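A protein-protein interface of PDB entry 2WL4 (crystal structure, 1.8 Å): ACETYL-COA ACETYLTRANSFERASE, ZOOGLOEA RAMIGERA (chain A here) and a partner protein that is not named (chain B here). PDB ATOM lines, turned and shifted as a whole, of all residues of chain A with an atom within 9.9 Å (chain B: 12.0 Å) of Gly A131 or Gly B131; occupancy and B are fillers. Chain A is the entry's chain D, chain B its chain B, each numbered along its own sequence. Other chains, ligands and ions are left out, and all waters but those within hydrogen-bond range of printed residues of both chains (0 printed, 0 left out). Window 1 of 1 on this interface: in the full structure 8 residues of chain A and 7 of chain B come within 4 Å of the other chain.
The backbone carbonyl oxygen of Leu B128 is in hydrogen-bond range of the backbone NH of Val A132 (3.0 Å). The guanidinium group (NH1) of Arg B129 sits at hydrogen-bond distance from the backbone carbonyl oxygen (O) of Lys A133. N of Val B132 lies within hydrogen-bond range of O of Leu A128, at 2.9 Å. NH1 of Arg A129 sits at hydrogen-bond distance from O of Lys B133.
The backbone carbonyl oxygen of Gly A130 sits at hydrogen-bond distance from the side-chain amino group of Lys A133, 3.0 Å away.
Among the printed residues, pairs that only touch across the chains: Leu A128 with Gly B131 (3.0 Å), Gly A131 with Gly B131 (3.3 Å), Arg A129 with Val B132 (3.3 Å), Gly A131 with Leu B128 (3.4 Å), Arg A129 with Met B134 (3.5 Å), Met A134 with Arg B129 (3.6 Å), Arg A129 with Gly B131 (3.7 Å), Leu A128 with Phe B137 (3.7 Å), Phe A137 with Leu B128 (3.8 Å), Val A132 with Arg B129 (3.8 Å) and Gly A130 with Gly B131 (3.9 Å).
No residue of chain B comes within 4 Å of His A127. Of chain B, only Gly B131 (3.0 Å), Val B132 (2.9 Å) and Phe B137 (3.7 Å) come within 4 Å of Leu A128. Of the printed residues of chain B, Arg A129 touches Gly B131 (3.7 Å), Val B132 (3.3 Å), Lys B133 (2.8 Å) and Met B134 (3.5 Å). Gly A130 touches just one residue of chain B: Gly B131 (3.9 Å). Of chain B, only Leu B128 (3.4 Å) and Gly B131 (3.3 Å) come within 4 Å of Gly A131. Of chain B, only Leu B128 (3.0 Å) and Arg B129 (3.8 Å) come within 4 Å of Val A132. Of chain B, only Arg B129 comes within 4 Å of Lys A133. Printed residues of chain B within 4 Å of Met A134: Arg B129. Gly A135 touches none of the printed residues of chain B. Of the printed residues of chain B, Phe A137 touches Leu B128 (3.8 Å). His B127 touches none of the printed residues of chain A. Printed residues of chain A within 4 Å of Leu B128: Gly A131, Val A132 and Phe A137. No residue of chain A comes within 4 Å of Gly B130. Gly B131 touches just these residues of chain A: Leu A128, Arg A129, Gly A130 and Gly A131. Val B132 touches just these residues of chain A: Leu A128 (2.9 Å) and Arg A129 (3.3 Å). Of the printed residues of chain A, Met B134 touches Arg A129 (3.5 Å). The nearest residue of chain A that does not touch Gly B131 is Val A132 (5.0 Å).
Hydrophobic or aromatic side chains of chain B that line the printed part of chain A: Leu B128, Met B134 and Phe B137. Of the 12 printed residues of chain A, 8 touch a printed residue of chain B. Hydrophobic or aromatic side chains of chain A that line the printed part of chain B: Leu A128 and Phe A137.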
ATOM      1  N   ALA A 126      26.443 -24.012 -23.389  1.00  0.00           N
ATOM      2  CA  ALA A 126      27.360 -23.672 -22.327  1.00  0.00           C
ATOM      3  C   ALA A 126      26.600 -23.054 -21.176  1.00  0.00           C
ATOM      4  O   ALA A 126      25.550 -22.438 -21.373  1.00  0.00           O
ATOM      5  CB  ALA A 126      28.408 -22.694 -22.827  1.00  0.00           C
ATOM      6  N   HIS A 127      27.143 -23.199 -19.974  1.00  0.00           N
ATOM      7  CA  HIS A 127      26.564 -22.529 -18.830  1.00  0.00           C
ATOM      8  C   HIS A 127      27.140 -21.122 -18.719  1.00  0.00           C
ATOM      9  O   HIS A 127      28.330 -20.954 -18.470  1.00  0.00           O
ATOM     10  CB  HIS A 127      26.801 -23.324 -17.547  1.00  0.00           C
ATOM     11  CG  HIS A 127      26.215 -22.676 -16.331  1.00  0.00           C
ATOM     12  ND1 HIS A 127      26.985 -22.219 -15.288  1.00  0.00           N
ATOM     13  CD2 HIS A 127      24.931 -22.382 -16.013  1.00  0.00           C
ATOM     14  CE1 HIS A 127      26.200 -21.683 -14.367  1.00  0.00           C
ATOM     15  NE2 HIS A 127      24.952 -21.768 -14.785  1.00  0.00           N
ATOM     16  N   LEU A 128      26.276 -20.122 -18.886  1.00  0.00           N
ATOM     17  CA  LEU A 128      26.692 -18.724 -18.962  1.00  0.00           C
ATOM     18  C   LEU A 128      25.935 -17.872 -17.960  1.00  0.00           C
ATOM     19  O   LEU A 128      26.094 -16.651 -17.910  1.00  0.00           O
ATOM     20  CB  LEU A 128      26.445 -18.198 -20.381  1.00  0.00           C
ATOM     21  CG  LEU A 128      26.891 -19.150 -21.493  1.00  0.00           C
ATOM     22  CD1 LEU A 128      26.412 -18.657 -22.857  1.00  0.00           C
ATOM     23  CD2 LEU A 128      28.407 -19.342 -21.472  1.00  0.00           C
ATOM     24  N   ARG A 129      25.112 -18.527 -17.151  1.00  0.00           N
ATOM     25  CA  ARG A 129      24.293 -17.827 -16.176  1.00  0.00           C
ATOM     26  C   ARG A 129      25.172 -17.102 -15.166  1.00  0.00           C
ATOM     27  O   ARG A 129      24.885 -15.969 -14.775  1.00  0.00           O
ATOM     28  CB  ARG A 129      23.369 -18.815 -15.465  1.00  0.00           C
ATOM     29  CG  ARG A 129      22.003 -18.256 -15.153  1.00  0.00           C
ATOM     30  CD  ARG A 129      21.083 -19.336 -14.596  1.00  0.00           C
ATOM     31  NE  ARG A 129      20.765 -20.379 -15.566  1.00  0.00           N
ATOM     32  CZ  ARG A 129      19.927 -20.229 -16.589  1.00  0.00           C
ATOM     33  NH1 ARG A 129      19.333 -19.060 -16.807  1.00  0.00           N
ATOM     34  NH2 ARG A 129      19.700 -21.248 -17.415  1.00  0.00           N
ATOM     35  N   GLY A 130      26.242 -17.765 -14.742  1.00  0.00           N
ATOM     36  CA  GLY A 130      27.207 -17.158 -13.845  1.00  0.00           C
ATOM     37  C   GLY A 130      28.159 -16.244 -14.590  1.00  0.00           C
ATOM     38  O   GLY A 130      28.709 -15.307 -14.020  1.00  0.00           O
ATOM     39  N   GLY A 131      28.350 -16.520 -15.874  1.00  0.00           N
ATOM     40  CA  GLY A 131      29.221 -15.707 -16.702  1.00  0.00           C
ATOM     41  C   GLY A 131      30.563 -16.353 -16.979  1.00  0.00           C
ATOM     42  O   GLY A 131      30.880 -17.425 -16.457  1.00  0.00           O
ATOM     43  N   VAL A 132      31.353 -15.691 -17.817  1.00  0.00           N
ATOM     44  CA  VAL A 132      32.688 -16.150 -18.165  1.00  0.00           C
ATOM     45  C   VAL A 132      33.609 -14.944 -18.042  1.00  0.00           C
ATOM     46  O   VAL A 132      33.904 -14.270 -19.029  1.00  0.00           O
ATOM     47  CB  VAL A 132      32.715 -16.698 -19.601  1.00  0.00           C
ATOM     48  CG1 VAL A 132      34.086 -17.269 -19.943  1.00  0.00           C
ATOM     49  CG2 VAL A 132      31.636 -17.758 -19.774  1.00  0.00           C
ATOM     50  N   LYS A 133      34.050 -14.679 -16.818  1.00  0.00           N
ATOM     51  CA  LYS A 133      34.727 -13.431 -16.475  1.00  0.00           C
ATOM     52  C   LYS A 133      35.843 -13.008 -17.435  1.00  0.00           C
ATOM     53  O   LYS A 133      35.965 -11.833 -17.754  1.00  0.00           O
ATOM     54  CB  LYS A 133      35.253 -13.493 -15.042  1.00  0.00           C
ATOM     55  CG  LYS A 133      34.158 -13.638 -13.996  1.00  0.00           C
ATOM     56  CD  LYS A 133      33.164 -12.494 -14.081  1.00  0.00           C
ATOM     57  CE  LYS A 133      32.024 -12.683 -13.098  1.00  0.00           C
ATOM     58  NZ  LYS A 133      31.333 -13.980 -13.315  1.00  0.00           N
ATOM     59  N   MET A 134      36.641 -13.967 -17.896  1.00  0.00           N
ATOM     60  CA  MET A 134      37.797 -13.675 -18.742  1.00  0.00           C
ATOM     61  C   MET A 134      38.421 -14.956 -19.286  1.00  0.00           C
ATOM     62  O   MET A 134      38.566 -15.927 -18.551  1.00  0.00           O
ATOM     63  CB  MET A 134      38.836 -12.913 -17.919  1.00  0.00           C
ATOM     64  CG  MET A 134      40.262 -13.014 -18.413  1.00  0.00           C
ATOM     65  SD  MET A 134      41.378 -12.067 -17.346  1.00  0.00           S
ATOM     66  CE  MET A 134      41.155 -12.917 -15.784  1.00  0.00           C
ATOM     67  N   GLY A 135      38.804 -14.956 -20.561  1.00  0.00           N
ATOM     68  CA  GLY A 135      39.488 -16.095 -21.157  1.00  0.00           C
ATOM     69  C   GLY A 135      38.592 -16.948 -22.041  1.00  0.00           C
ATOM     70  O   GLY A 135      37.372 -16.855 -21.970  1.00  0.00           O
ATOM     71  N   ASP A 136      39.199 -17.759 -22.894  1.00  0.00           N
ATOM     72  CA  ASP A 136      38.424 -18.566 -23.841  1.00  0.00           C
ATOM     73  C   ASP A 136      37.629 -19.658 -23.113  1.00  0.00           C
ATOM     74  O   ASP A 136      37.977 -20.042 -21.996  1.00  0.00           O
ATOM     75  CB  ASP A 136      39.351 -19.201 -24.860  1.00  0.00           C
ATOM     76  CG  ASP A 136      40.109 -18.186 -25.649  1.00  0.00           C
ATOM     77  OD1 ASP A 136      39.791 -16.985 -25.512  1.00  0.00           O
ATOM     78  OD2 ASP A 136      41.024 -18.588 -26.391  1.00  0.00           O
ATOM     79  N   PHE A 137      36.562 -20.145 -23.744  1.00  0.00           N
ATOM     80  CA  PHE A 137      35.779 -21.258 -23.193  1.00  0.00           C
ATOM     81  C   PHE A 137      35.221 -22.152 -24.300  1.00  0.00           C
ATOM     82  O   PHE A 137      35.444 -21.885 -25.487  1.00  0.00           O
ATOM     83  CB  PHE A 137      34.651 -20.752 -22.288  1.00  0.00           C
ATOM     84  CG  PHE A 137      33.475 -20.174 -23.026  1.00  0.00           C
ATOM     85  CD1 PHE A 137      32.390 -20.972 -23.367  1.00  0.00           C
ATOM     86  CD2 PHE A 137      33.445 -18.836 -23.368  1.00  0.00           C
ATOM     87  CE1 PHE A 137      31.304 -20.444 -24.038  1.00  0.00           C
ATOM     88  CE2 PHE A 137      32.364 -18.298 -24.035  1.00  0.00           C
ATOM     89  CZ  PHE A 137      31.290 -19.106 -24.375  1.00  0.00           C
ATOM     90  N   ALA B 126      29.294 -12.323 -28.522  1.00  0.00           N
ATOM     91  CA  ALA B 126      28.352 -12.054 -27.447  1.00  0.00           C
ATOM     92  C   ALA B 126      29.107 -11.615 -26.211  1.00  0.00           C
ATOM     93  O   ALA B 126      30.140 -12.178 -25.893  1.00  0.00           O
ATOM     94  CB  ALA B 126      27.508 -13.299 -27.141  1.00  0.00           C
ATOM     95  N   HIS B 127      28.579 -10.609 -25.524  1.00  0.00           N
ATOM     96  CA  HIS B 127      29.140 -10.179 -24.247  1.00  0.00           C
ATOM     97  C   HIS B 127      28.611 -11.073 -23.144  1.00  0.00           C
ATOM     98  O   HIS B 127      27.428 -11.029 -22.830  1.00  0.00           O
ATOM     99  CB  HIS B 127      28.772  -8.724 -23.949  1.00  0.00           C
ATOM    100  CG  HIS B 127      29.225  -8.253 -22.604  1.00  0.00           C
ATOM    101  ND1 HIS B 127      28.356  -7.727 -21.657  1.00  0.00           N
ATOM    102  CD2 HIS B 127      30.440  -8.273 -22.007  1.00  0.00           C
ATOM    103  CE1 HIS B 127      29.027  -7.405 -20.575  1.00  0.00           C
ATOM    104  NE2 HIS B 127      30.303  -7.734 -20.754  1.00  0.00           N
ATOM    105  N   LEU B 128      29.505 -11.858 -22.549  1.00  0.00           N
ATOM    106  CA  LEU B 128      29.129 -12.928 -21.636  1.00  0.00           C
ATOM    107  C   LEU B 128      29.785 -12.819 -20.258  1.00  0.00           C
ATOM    108  O   LEU B 128      29.730 -13.773 -19.475  1.00  0.00           O
ATOM    109  CB  LEU B 128      29.501 -14.270 -22.261  1.00  0.00           C
ATOM    110  CG  LEU B 128      28.838 -14.579 -23.612  1.00  0.00           C
ATOM    111  CD1 LEU B 128      29.357 -15.875 -24.176  1.00  0.00           C
ATOM    112  CD2 LEU B 128      27.328 -14.647 -23.435  1.00  0.00           C
ATOM    113  N   ARG B 129      30.401 -11.669 -19.967  1.00  0.00           N
ATOM    114  CA  ARG B 129      31.135 -11.472 -18.713  1.00  0.00           C
ATOM    115  C   ARG B 129      30.256 -11.340 -17.479  1.00  0.00           C
ATOM    116  O   ARG B 129      30.591 -11.874 -16.418  1.00  0.00           O
ATOM    117  CB  ARG B 129      32.067 -10.255 -18.799  1.00  0.00           C
ATOM    118  CG  ARG B 129      33.354 -10.560 -19.520  1.00  0.00           C
ATOM    119  CD  ARG B 129      34.392  -9.442 -19.389  1.00  0.00           C
ATOM    120  NE  ARG B 129      34.933  -9.200 -20.712  1.00  0.00           N
ATOM    121  CZ  ARG B 129      35.879  -9.939 -21.280  1.00  0.00           C
ATOM    122  NH1 ARG B 129      36.404 -10.973 -20.626  1.00  0.00           N
ATOM    123  NH2 ARG B 129      36.275  -9.661 -22.515  1.00  0.00           N
ATOM    124  N   GLY B 130      29.147 -10.619 -17.615  1.00  0.00           N
ATOM    125  CA  GLY B 130      28.232 -10.427 -16.505  1.00  0.00           C
ATOM    126  C   GLY B 130      27.282 -11.594 -16.348  1.00  0.00           C
ATOM    127  O   GLY B 130      26.382 -11.560 -15.509  1.00  0.00           O
ATOM    128  N   GLY B 131      27.487 -12.636 -17.150  1.00  0.00           N
ATOM    129  CA  GLY B 131      26.589 -13.775 -17.157  1.00  0.00           C
ATOM    130  C   GLY B 131      25.161 -13.385 -17.496  1.00  0.00           C
ATOM    131  O   GLY B 131      24.686 -12.321 -17.102  1.00  0.00           O
ATOM    132  N   VAL B 132      24.472 -14.240 -18.241  1.00  0.00           N
ATOM    133  CA  VAL B 132      23.069 -13.995 -18.560  1.00  0.00           C
ATOM    134  C   VAL B 132      22.175 -14.755 -17.583  1.00  0.00           C
ATOM    135  O   VAL B 132      21.989 -15.966 -17.700  1.00  0.00           O
ATOM    136  CB  VAL B 132      22.744 -14.365 -20.023  1.00  0.00           C
ATOM    137  CG1 VAL B 132      21.242 -14.417 -20.242  1.00  0.00           C
ATOM    138  CG2 VAL B 132      23.391 -13.359 -20.971  1.00  0.00           C
ATOM    139  N   LYS B 133      21.640 -14.024 -16.611  1.00  0.00           N
ATOM    140  CA  LYS B 133      20.915 -14.617 -15.496  1.00  0.00           C
ATOM    141  C   LYS B 133      19.775 -15.520 -15.951  1.00  0.00           C
ATOM    142  O   LYS B 133      19.618 -16.618 -15.426  1.00  0.00           O
ATOM    143  CB  LYS B 133      20.411 -13.528 -14.546  1.00  0.00           C
ATOM    144  CG  LYS B 133      21.490 -12.508 -14.186  1.00  0.00           C
ATOM    145  CD  LYS B 133      20.935 -11.320 -13.408  1.00  0.00           C
ATOM    146  CE  LYS B 133      21.770 -10.063 -13.646  1.00  0.00           C
ATOM    147  NZ  LYS B 133      23.194 -10.214 -13.227  1.00  0.00           N
ATOM    148  N   MET B 134      18.986 -15.063 -16.921  1.00  0.00           N
ATOM    149  CA  MET B 134      17.936 -15.903 -17.505  1.00  0.00           C
ATOM    150  C   MET B 134      17.273 -15.242 -18.713  1.00  0.00           C
ATOM    151  O   MET B 134      17.139 -14.018 -18.765  1.00  0.00           O
ATOM    152  CB  MET B 134      16.889 -16.298 -16.454  1.00  0.00           C
ATOM    153  CG  MET B 134      15.621 -15.454 -16.441  1.00  0.00           C
ATOM    154  SD  MET B 134      14.551 -15.938 -15.069  1.00  0.00           S
ATOM    155  CE  MET B 134      12.965 -15.280 -15.567  1.00  0.00           C
ATOM    156  N   GLY B 135      16.862 -16.062 -19.679  1.00  0.00           N
ATOM    157  CA  GLY B 135      16.276 -15.576 -20.920  1.00  0.00           C
ATOM    158  C   GLY B 135      17.230 -15.689 -22.099  1.00  0.00           C
ATOM    159  O   GLY B 135      18.441 -15.782 -21.921  1.00  0.00           O
ATOM    160  N   ASP B 136      16.689 -15.678 -23.312  1.00  0.00           N
ATOM    161  CA  ASP B 136      17.522 -15.833 -24.504  1.00  0.00           C
ATOM    162  C   ASP B 136      18.423 -14.626 -24.742  1.00  0.00           C
ATOM    163  O   ASP B 136      18.180 -13.535 -24.214  1.00  0.00           O
ATOM    164  CB  ASP B 136      16.656 -16.092 -25.744  1.00  0.00           C
ATOM    165  CG  ASP B 136      15.816 -17.350 -25.615  1.00  0.00           C
ATOM    166  OD1 ASP B 136      16.107 -18.168 -24.722  1.00  0.00           O
ATOM    167  OD2 ASP B 136      14.863 -17.522 -26.406  1.00  0.00           O
ATOM    168  N   PHE B 137      19.470 -14.839 -25.534  1.00  0.00           N
ATOM    169  CA  PHE B 137      20.352 -13.764 -25.971  1.00  0.00           C
ATOM    170  C   PHE B 137      20.951 -14.135 -27.324  1.00  0.00           C
ATOM    171  O   PHE B 137      21.121 -15.310 -27.634  1.00  0.00           O
ATOM    172  CB  PHE B 137      21.464 -13.518 -24.951  1.00  0.00           C
ATOM    173  CG  PHE B 137      22.595 -14.512 -25.028  1.00  0.00           C
ATOM    174  CD1 PHE B 137      22.638 -15.593 -24.175  1.00  0.00           C
ATOM    175  CD2 PHE B 137      23.623 -14.352 -25.949  1.00  0.00           C
ATOM    176  CE1 PHE B 137      23.679 -16.506 -24.236  1.00  0.00           C
ATOM    177  CE2 PHE B 137      24.664 -15.267 -26.017  1.00  0.00           C
ATOM    178  CZ  PHE B 137      24.693 -16.339 -25.164  1.00  0.00           C
ATOM    179  N   LYS B 138      21.292 -13.131 -28.118  1.00  0.00           N
ATOM    180  CA  LYS B 138      21.787 -13.377 -29.470  1.00  0.00           C
ATOM    181  C   LYS B 138      23.300 -13.625 -29.519  1.00  0.00           C
ATOM    182  O   LYS B 138      24.054 -13.045 -28.751  1.00  0.00           O
ATOM    183  CB  LYS B 138      21.455 -12.173 -30.354  1.00  0.00           C
ATOM    184  CG  LYS B 138      20.503 -11.176 -29.703  1.00  0.00           C
ATOM    185  CD  LYS B 138      20.121 -10.047 -30.645  1.00  0.00           C
ATOM    186  CE  LYS B 138      18.940 -10.422 -31.532  1.00  0.00           C
ATOM    187  NZ  LYS B 138      17.644 -10.418 -30.792  1.00  0.00           N
